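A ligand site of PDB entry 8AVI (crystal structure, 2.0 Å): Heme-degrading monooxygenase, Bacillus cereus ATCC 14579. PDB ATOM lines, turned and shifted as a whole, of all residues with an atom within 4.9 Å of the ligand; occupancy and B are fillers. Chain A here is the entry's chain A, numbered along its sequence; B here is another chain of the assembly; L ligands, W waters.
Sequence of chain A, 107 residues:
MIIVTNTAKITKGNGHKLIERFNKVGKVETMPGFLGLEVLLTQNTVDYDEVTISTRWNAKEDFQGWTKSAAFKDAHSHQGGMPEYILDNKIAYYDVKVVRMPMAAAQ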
ATOM      1  N   VAL A   4      28.060 -20.475  15.357  1.00  0.00           N
ATOM      2  CA  VAL A   4      28.901 -19.321  15.657  1.00  0.00           C
ATOM      3  C   VAL A   4      28.657 -18.938  17.104  1.00  0.00           C
ATOM      4  O   VAL A   4      27.512 -18.750  17.507  1.00  0.00           O
ATOM      5  CB  VAL A   4      28.586 -18.140  14.734  1.00  0.00           C
ATOM      6  CG1 VAL A   4      29.518 -16.991  15.036  1.00  0.00           C
ATOM      7  CG2 VAL A   4      28.706 -18.561  13.265  1.00  0.00           C
ATOM      8  N   ASN A   6      29.690 -16.440  20.528  1.00  0.00           N
ATOM      9  CA  ASN A   6      30.292 -15.256  21.119  1.00  0.00           C
ATOM     10  C   ASN A   6      30.339 -15.519  22.621  1.00  0.00           C
ATOM     11  O   ASN A   6      29.291 -15.646  23.265  1.00  0.00           O
ATOM     12  CB  ASN A   6      29.470 -14.012  20.787  1.00  0.00           C
ATOM     13  CG  ASN A   6      30.187 -12.719  21.109  1.00  0.00           C
ATOM     14  OD1 ASN A   6      31.411 -12.666  21.147  1.00  0.00           O
ATOM     15  ND2 ASN A   6      29.415 -11.667  21.328  1.00  0.00           N
ATOM     16  N   LEU A  18      23.841  -9.567  30.954  1.00  0.00           N
ATOM     17  CA  LEU A  18      23.947  -9.866  29.539  1.00  0.00           C
ATOM     18  C   LEU A  18      22.869 -10.848  29.113  1.00  0.00           C
ATOM     19  O   LEU A  18      22.340 -10.754  28.000  1.00  0.00           O
ATOM     20  CB  LEU A  18      25.341 -10.406  29.237  1.00  0.00           C
ATOM     21  CG  LEU A  18      25.562 -10.661  27.758  1.00  0.00           C
ATOM     22  CD1 LEU A  18      25.394  -9.380  26.973  1.00  0.00           C
ATOM     23  CD2 LEU A  18      26.938 -11.232  27.590  1.00  0.00           C
ATOM     24  N   ARG A  21      19.564  -9.225  28.302  1.00  0.00           N
ATOM     25  CA  ARG A  21      19.545  -8.491  27.048  1.00  0.00           C
ATOM     26  C   ARG A  21      19.198  -9.374  25.849  1.00  0.00           C
ATOM     27  O   ARG A  21      18.750  -8.868  24.817  1.00  0.00           O
ATOM     28  CB  ARG A  21      20.909  -7.839  26.829  1.00  0.00           C
ATOM     29  CG  ARG A  21      20.888  -6.736  25.785  1.00  0.00           C
ATOM     30  CD  ARG A  21      22.132  -5.849  25.871  1.00  0.00           C
ATOM     31  NE  ARG A  21      22.379  -5.337  27.218  1.00  0.00           N
ATOM     32  CZ  ARG A  21      23.414  -4.579  27.538  1.00  0.00           C
ATOM     33  NH1 ARG A  21      24.309  -4.205  26.636  1.00  0.00           N
ATOM     34  NH2 ARG A  21      23.559  -4.193  28.811  1.00  0.00           N
ATOM     35  N   PHE A  22      19.425 -10.686  25.956  1.00  0.00           N
ATOM     36  CA  PHE A  22      19.051 -11.616  24.907  1.00  0.00           C
ATOM     37  C   PHE A  22      17.727 -12.315  25.180  1.00  0.00           C
ATOM     38  O   PHE A  22      17.213 -13.004  24.294  1.00  0.00           O
ATOM     39  CB  PHE A  22      20.169 -12.653  24.709  1.00  0.00           C
ATOM     40  CG  PHE A  22      21.324 -12.096  23.939  1.00  0.00           C
ATOM     41  CD1 PHE A  22      22.332 -11.403  24.593  1.00  0.00           C
ATOM     42  CD2 PHE A  22      21.372 -12.197  22.567  1.00  0.00           C
ATOM     43  CE1 PHE A  22      23.376 -10.861  23.898  1.00  0.00           C
ATOM     44  CE2 PHE A  22      22.419 -11.642  21.866  1.00  0.00           C
ATOM     45  CZ  PHE A  22      23.416 -10.977  22.540  1.00  0.00           C
ATOM     46  N   GLY A  26      13.687 -11.517  18.916  1.00  0.00           N
ATOM     47  CA  GLY A  26      14.401 -10.526  18.131  1.00  0.00           C
ATOM     48  C   GLY A  26      14.246 -10.752  16.640  1.00  0.00           C
ATOM     49  O   GLY A  26      13.321 -11.434  16.203  1.00  0.00           O
ATOM     50  N   LYS A  27      15.169 -10.212  15.854  1.00  0.00           N
ATOM     51  CA  LYS A  27      15.108 -10.338  14.412  1.00  0.00           C
ATOM     52  C   LYS A  27      15.980 -11.463  13.846  1.00  0.00           C
ATOM     53  O   LYS A  27      15.658 -11.995  12.772  1.00  0.00           O
ATOM     54  CB  LYS A  27      15.522  -9.012  13.754  1.00  0.00           C
ATOM     55  CG  LYS A  27      14.420  -7.954  13.765  1.00  0.00           C
ATOM     56  CD  LYS A  27      13.198  -8.417  12.981  1.00  0.00           C
ATOM     57  CE  LYS A  27      11.983  -8.639  13.882  1.00  0.00           C
ATOM     58  NZ  LYS A  27      10.760  -9.075  13.117  1.00  0.00           N
ATOM     59  N   VAL A  28      17.071 -11.833  14.533  1.00  0.00           N
ATOM     60  CA  VAL A  28      17.953 -12.836  13.940  1.00  0.00           C
ATOM     61  C   VAL A  28      17.192 -14.124  13.654  1.00  0.00           C
ATOM     62  O   VAL A  28      17.503 -14.825  12.680  1.00  0.00           O
ATOM     63  CB  VAL A  28      19.201 -13.085  14.824  1.00  0.00           C
ATOM     64  CG1 VAL A  28      18.828 -13.710  16.166  1.00  0.00           C
ATOM     65  CG2 VAL A  28      20.223 -13.958  14.076  1.00  0.00           C
ATOM     66  N   GLU A  29      16.139 -14.397  14.440  1.00  0.00           N
ATOM     67  CA  GLU A  29      15.311 -15.593  14.300  1.00  0.00           C
ATOM     68  C   GLU A  29      14.538 -15.643  12.982  1.00  0.00           C
ATOM     69  O   GLU A  29      14.028 -16.705  12.622  1.00  0.00           O
ATOM     70  CB  GLU A  29      14.313 -15.665  15.453  1.00  0.00           C
ATOM     71  CG  GLU A  29      14.961 -15.761  16.821  1.00  0.00           C
ATOM     72  CD  GLU A  29      14.951 -14.446  17.598  1.00  0.00           C
ATOM     73  OE1 GLU A  29      15.639 -13.487  17.181  1.00  0.00           O
ATOM     74  OE2 GLU A  29      14.283 -14.407  18.651  1.00  0.00           O
ATOM     75  N   LEU A  37      19.143 -20.031  18.398  1.00  0.00           N
ATOM     76  CA  LEU A  37      20.054 -19.256  19.212  1.00  0.00           C
ATOM     77  C   LEU A  37      19.877 -19.712  20.658  1.00  0.00           C
ATOM     78  O   LEU A  37      18.750 -19.905  21.106  1.00  0.00           O
ATOM     79  CB  LEU A  37      19.795 -17.737  19.081  1.00  0.00           C
ATOM     80  CG  LEU A  37      20.644 -16.788  19.905  1.00  0.00           C
ATOM     81  CD1 LEU A  37      20.700 -15.432  19.245  1.00  0.00           C
ATOM     82  CD2 LEU A  37      20.084 -16.652  21.321  1.00  0.00           C
ATOM     83  N   THR A  55      24.749 -19.245  18.011  1.00  0.00           N
ATOM     84  CA  THR A  55      23.776 -19.286  16.917  1.00  0.00           C
ATOM     85  C   THR A  55      24.150 -20.399  15.932  1.00  0.00           C
ATOM     86  O   THR A  55      25.335 -20.640  15.665  1.00  0.00           O
ATOM     87  CB  THR A  55      23.677 -17.935  16.204  1.00  0.00           C
ATOM     88  OG1 THR A  55      24.914 -17.646  15.539  1.00  0.00           O
ATOM     89  CG2 THR A  55      23.387 -16.842  17.206  1.00  0.00           C
ATOM     90  N   PHE A  63      24.784 -17.077   7.914  1.00  0.00           N
ATOM     91  CA  PHE A  63      25.272 -16.189   8.967  1.00  0.00           C
ATOM     92  C   PHE A  63      25.791 -14.889   8.372  1.00  0.00           C
ATOM     93  O   PHE A  63      25.572 -13.813   8.932  1.00  0.00           O
ATOM     94  CB  PHE A  63      26.385 -16.875   9.745  1.00  0.00           C
ATOM     95  CG  PHE A  63      27.098 -15.977  10.690  1.00  0.00           C
ATOM     96  CD1 PHE A  63      26.501 -15.571  11.886  1.00  0.00           C
ATOM     97  CD2 PHE A  63      28.388 -15.545  10.420  1.00  0.00           C
ATOM     98  CE1 PHE A  63      27.172 -14.750  12.771  1.00  0.00           C
ATOM     99  CE2 PHE A  63      29.053 -14.712  11.294  1.00  0.00           C
ATOM    100  CZ  PHE A  63      28.450 -14.326  12.480  1.00  0.00           C
ATOM    101  N   TRP A  66      23.111 -12.527   7.491  1.00  0.00           N
ATOM    102  CA  TRP A  66      22.549 -11.800   8.617  1.00  0.00           C
ATOM    103  C   TRP A  66      23.453 -10.638   9.027  1.00  0.00           C
ATOM    104  O   TRP A  66      22.949  -9.551   9.300  1.00  0.00           O
ATOM    105  CB  TRP A  66      22.301 -12.713   9.808  1.00  0.00           C
ATOM    106  CG  TRP A  66      21.928 -11.929  11.022  1.00  0.00           C
ATOM    107  CD1 TRP A  66      20.869 -11.055  11.154  1.00  0.00           C
ATOM    108  CD2 TRP A  66      22.607 -11.911  12.266  1.00  0.00           C
ATOM    109  NE1 TRP A  66      20.858 -10.506  12.403  1.00  0.00           N
ATOM    110  CE2 TRP A  66      21.914 -11.013  13.122  1.00  0.00           C
ATOM    111  CE3 TRP A  66      23.732 -12.575  12.760  1.00  0.00           C
ATOM    112  CZ2 TRP A  66      22.317 -10.775  14.423  1.00  0.00           C
ATOM    113  CZ3 TRP A  66      24.128 -12.321  14.073  1.00  0.00           C
ATOM    114  CH2 TRP A  66      23.422 -11.434  14.872  1.00  0.00           C
ATOM    115  N   PHE A  72      20.713  -6.586  11.676  1.00  0.00           N
ATOM    116  CA  PHE A  72      21.963  -6.649  12.418  1.00  0.00           C
ATOM    117  C   PHE A  72      22.465  -5.243  12.762  1.00  0.00           C
ATOM    118  O   PHE A  72      23.010  -5.030  13.861  1.00  0.00           O
ATOM    119  CB  PHE A  72      23.029  -7.415  11.646  1.00  0.00           C
ATOM    120  CG  PHE A  72      24.355  -7.474  12.337  1.00  0.00           C
ATOM    121  CD1 PHE A  72      24.596  -8.423  13.327  1.00  0.00           C
ATOM    122  CD2 PHE A  72      25.378  -6.599  12.009  1.00  0.00           C
ATOM    123  CE1 PHE A  72      25.821  -8.480  13.973  1.00  0.00           C
ATOM    124  CE2 PHE A  72      26.599  -6.654  12.642  1.00  0.00           C
ATOM    125  CZ  PHE A  72      26.829  -7.594  13.629  1.00  0.00           C
ATOM    126  N   ALA A  75      20.117  -4.048  15.554  1.00  0.00           N
ATOM    127  CA  ALA A  75      20.438  -4.737  16.801  1.00  0.00           C
ATOM    128  C   ALA A  75      21.864  -4.471  17.270  1.00  0.00           C
ATOM    129  O   ALA A  75      22.238  -4.959  18.349  1.00  0.00           O
ATOM    130  CB  ALA A  75      20.210  -6.241  16.653  1.00  0.00           C
ATOM    131  N   HIS A  76      22.664  -3.738  16.499  1.00  0.00           N
ATOM    132  CA  HIS A  76      23.974  -3.267  16.931  1.00  0.00           C
ATOM    133  C   HIS A  76      24.048  -1.743  16.905  1.00  0.00           C
ATOM    134  O   HIS A  76      25.096  -1.163  16.618  1.00  0.00           O
ATOM    135  CB  HIS A  76      25.083  -3.870  16.068  1.00  0.00           C
ATOM    136  CG  HIS A  76      25.513  -5.239  16.509  1.00  0.00           C
ATOM    137  ND1 HIS A  76      26.820  -5.528  16.855  1.00  0.00           N
ATOM    138  CD2 HIS A  76      24.817  -6.391  16.659  1.00  0.00           C
ATOM    139  CE1 HIS A  76      26.897  -6.803  17.199  1.00  0.00           C
ATOM    140  NE2 HIS A  76      25.709  -7.352  17.084  1.00  0.00           N
ATOM    141  N   GLN A  79      23.284  -0.296  21.712  1.00  0.00           N
ATOM    142  CA  GLN A  79      23.760  -1.248  22.715  1.00  0.00           C
ATOM    143  C   GLN A  79      24.295  -0.561  23.969  1.00  0.00           C
ATOM    144  O   GLN A  79      24.642  -1.257  24.932  1.00  0.00           O
ATOM    145  CB  GLN A  79      24.863  -2.130  22.129  1.00  0.00           C
ATOM    146  CG  GLN A  79      24.601  -2.665  20.731  1.00  0.00           C
ATOM    147  CD  GLN A  79      25.762  -3.491  20.219  1.00  0.00           C
ATOM    148  OE1 GLN A  79      26.154  -4.477  20.831  1.00  0.00           O
ATOM    149  NE2 GLN A  79      26.335  -3.074  19.091  1.00  0.00           N
ATOM    150  N   MET A  82      29.933  -1.488  24.382  1.00  0.00           N
ATOM    151  CA  MET A  82      30.292  -2.679  25.148  1.00  0.00           C
ATOM    152  C   MET A  82      30.216  -2.336  26.629  1.00  0.00           C
ATOM    153  O   MET A  82      30.911  -1.418  27.082  1.00  0.00           O
ATOM    154  CB  MET A  82      31.689  -3.172  24.779  1.00  0.00           C
ATOM    155  CG  MET A  82      32.003  -4.585  25.284  1.00  0.00           C
ATOM    156  SD  MET A  82      33.619  -5.211  24.746  1.00  0.00           S
ATOM    157  CE  MET A  82      33.482  -4.997  22.964  1.00  0.00           C
ATOM    158  N   ILE A  86      32.210  -6.232  30.935  1.00  0.00           N
ATOM    159  CA  ILE A  86      32.720  -7.192  29.980  1.00  0.00           C
ATOM    160  C   ILE A  86      34.238  -7.126  30.009  1.00  0.00           C
ATOM    161  O   ILE A  86      34.839  -6.145  29.561  1.00  0.00           O
ATOM    162  CB  ILE A  86      32.194  -6.929  28.566  1.00  0.00           C
ATOM    163  CG1 ILE A  86      30.703  -7.251  28.496  1.00  0.00           C
ATOM    164  CG2 ILE A  86      32.976  -7.730  27.528  1.00  0.00           C
ATOM    165  CD1 ILE A  86      30.136  -7.167  27.109  1.00  0.00           C
ATOM    166  N   ASN A  89      36.032 -10.960  25.278  1.00  0.00           N
ATOM    167  CA  ASN A  89      35.040 -11.485  24.342  1.00  0.00           C
ATOM    168  C   ASN A  89      35.744 -12.254  23.235  1.00  0.00           C
ATOM    169  O   ASN A  89      36.566 -11.684  22.520  1.00  0.00           O
ATOM    170  CB  ASN A  89      34.200 -10.354  23.751  1.00  0.00           C
ATOM    171  CG  ASN A  89      33.280 -10.834  22.667  1.00  0.00           C
ATOM    172  OD1 ASN A  89      33.583 -10.711  21.472  1.00  0.00           O
ATOM    173  ND2 ASN A  89      32.161 -11.417  23.056  1.00  0.00           N
ATOM    174  N   ILE A  91      35.116 -14.880  19.820  1.00  0.00           N
ATOM    175  CA  ILE A  91      34.195 -15.352  18.797  1.00  0.00           C
ATOM    176  C   ILE A  91      34.805 -16.591  18.156  1.00  0.00           C
ATOM    177  O   ILE A  91      35.987 -16.592  17.832  1.00  0.00           O
ATOM    178  CB  ILE A  91      33.921 -14.279  17.733  1.00  0.00           C
ATOM    179  CG1 ILE A  91      33.285 -13.047  18.381  1.00  0.00           C
ATOM    180  CG2 ILE A  91      33.087 -14.849  16.609  1.00  0.00           C
ATOM    181  CD1 ILE A  91      33.462 -11.762  17.577  1.00  0.00           C
ATOM    182  N   ARG B 100      16.016 -19.380  21.627  1.00  0.00           N
ATOM    183  CA  ARG B 100      15.227 -18.661  20.625  1.00  0.00           C
ATOM    184  C   ARG B 100      15.222 -19.452  19.327  1.00  0.00           C
ATOM    185  O   ARG B 100      16.262 -19.548  18.656  1.00  0.00           O
ATOM    186  CB  ARG B 100      15.771 -17.247  20.436  1.00  0.00           C
ATOM    187  CG  ARG B 100      15.291 -16.292  21.538  1.00  0.00           C
ATOM    188  CD  ARG B 100      16.215 -15.086  21.710  1.00  0.00           C
ATOM    189  NE  ARG B 100      16.222 -14.193  20.556  1.00  0.00           N
ATOM    190  CZ  ARG B 100      17.001 -13.118  20.452  1.00  0.00           C
ATOM    191  NH1 ARG B 100      17.764 -12.700  21.452  1.00  0.00           N
ATOM    192  NH2 ARG B 100      17.041 -12.459  19.302  1.00  0.00           N
HETATM  193  C1  LIG L   1      23.105  -7.944  19.621  1.00  0.00           C
HETATM  194  C2  LIG L   1      27.255  -7.232  21.998  1.00  0.00           C
HETATM  195  C3  LIG L   1      29.372  -9.536  18.287  1.00  0.00           C
HETATM  196  C4  LIG L   1      25.167 -11.888  17.695  1.00  0.00           C
HETATM  197  C5  LIG L   1      23.960  -7.531  20.624  1.00  0.00           C
HETATM  198  C6  LIG L   1      23.666  -6.870  21.892  1.00  0.00           C
HETATM  199  C7  LIG L   1      24.826  -6.687  22.530  1.00  0.00           C
HETATM  200  C8  LIG L   1      25.903  -7.224  21.717  1.00  0.00           C
HETATM  201  C9  LIG L   1      25.008  -6.018  23.913  1.00  0.00           C
HETATM  202  C10 LIG L   1      22.284  -6.434  22.443  1.00  0.00           C
HETATM  203  C11 LIG L   1      21.383  -5.788  21.402  1.00  0.00           C
HETATM  204  C12 LIG L   1      20.330  -6.790  20.995  1.00  0.00           C
HETATM  205  O1  LIG L   1      20.443  -7.976  21.387  1.00  0.00           O
HETATM  206  O2  LIG L   1      19.384  -6.394  20.255  1.00  0.00           O
HETATM  207  C13 LIG L   1      28.235  -7.685  21.145  1.00  0.00           C
HETATM  208  C14 LIG L   1      29.654  -7.415  21.206  1.00  0.00           C
HETATM  209  C15 LIG L   1      30.263  -8.033  20.189  1.00  0.00           C
HETATM  210  C16 LIG L   1      29.244  -8.743  19.417  1.00  0.00           C
HETATM  211  C17 LIG L   1      30.336  -6.530  22.285  1.00  0.00           C
HETATM  212  C18 LIG L   1      31.797  -7.965  19.930  1.00  0.00           C
HETATM  213  C19 LIG L   1      32.387  -8.560  18.885  1.00  0.00           C
HETATM  214  C20 LIG L   1      28.474 -10.547  17.953  1.00  0.00           C
HETATM  215  C21 LIG L   1      28.745 -11.866  17.405  1.00  0.00           C
HETATM  216  C22 LIG L   1      27.589 -12.518  17.264  1.00  0.00           C
HETATM  217  C23 LIG L   1      26.521 -11.636  17.690  1.00  0.00           C
HETATM  218  C24 LIG L   1      30.113 -12.472  17.054  1.00  0.00           C
HETATM  219  C25 LIG L   1      27.473 -13.963  16.696  1.00  0.00           C
HETATM  220  C26 LIG L   1      26.378 -14.716  16.879  1.00  0.00           C
HETATM  221  C27 LIG L   1      24.211 -11.017  18.169  1.00  0.00           C
HETATM  222  C28 LIG L   1      22.781 -11.241  18.223  1.00  0.00           C
HETATM  223  C29 LIG L   1      22.222 -10.156  18.751  1.00  0.00           C
HETATM  224  C30 LIG L   1      23.247  -9.187  19.049  1.00  0.00           C
HETATM  225  C31 LIG L   1      22.068 -12.522  17.753  1.00  0.00           C
HETATM  226  C32 LIG L   1      20.726  -9.945  18.999  1.00  0.00           C
HETATM  227  C33 LIG L   1      20.117  -9.550  17.676  1.00  0.00           C
HETATM  228  C34 LIG L   1      18.639  -9.786  17.794  1.00  0.00           C
HETATM  229  O3  LIG L   1      18.030 -10.106  16.757  1.00  0.00           O
HETATM  230  O4  LIG L   1      18.089  -9.667  18.914  1.00  0.00           O
HETATM  231  N1  LIG L   1      25.322  -7.724  20.567  1.00  0.00           N
HETATM  232  N2  LIG L   1      28.038  -8.499  20.041  1.00  0.00           N
HETATM  233  N3  LIG L   1      27.099 -10.450  18.103  1.00  0.00           N
HETATM  234  N4  LIG L   1      24.460  -9.755  18.683  1.00  0.00           N
HETATM  235 FE1  LIG L   1      26.229  -9.034  19.297  1.00  0.00          FE
HETATM  236  O   HOH W   1      18.312  -9.745  21.536  1.00  0.00           O
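NE2 of His 76 sits close to N4 of the ligand. The side-chain amide oxygen (OE1) of Gln 79 sits close to a nitrogen (N1) of the ligand (3.4 Å). Merely in contact with the ligand: Asn 6, Arg 21, Phe 22, Gly 26, Leu 37, Thr 55, Trp 66, Ala 75, Met 82, Asn 89 and Ile 91.
O3 of the ligand lies within hydrogen-bond range of N of Val 28 (3.0 Å). N of Lys 27 is in hydrogen-bond range of O3 of the ligand (3.0 Å). An oxygen (O4) of the ligand is in salt-bridge range of the guanidinium group (NH2) of Arg 100 of chain B (3.0 Å).
The side-chain amide nitrogen of Gln 79 lies close to a ring nitrogen (ND1) of His 76 (3.4 Å). O of Gln 79 lies within hydrogen-bond range of NH1 of Arg 21, at 3.4 Å. The backbone carbonyl oxygen (O) of Phe 22 is in hydrogen-bond range of the guanidinium group (NH1) of Arg 100 of chain B (2.9 Å). The backbone NH (N) of Arg 100 of chain B is in hydrogen-bond range of the backbone carbonyl oxygen (O) of Leu 37 (2.8 Å). The guanidinium group (NE) of Arg 100 of chain B is in salt-bridge range of the side-chain carboxylate (OE2) of Glu 29 (2.7 Å). ND2 of Asn 89 lies within hydrogen-bond range of OD1 of Asn 6. O of Thr 55 lies within hydrogen-bond range of N of Val 4 (2.7 Å). The backbone NH of Gly 26 sits at hydrogen-bond distance from the side-chain carboxylate of Glu 29, 3.0 Å away.
Water W1 lies within hydrogen-bond range of O4 of the ligand (2.6 Å), NH1 of Arg 100 of chain B (3.0 Å) and O of Arg 21 (3.4 Å).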
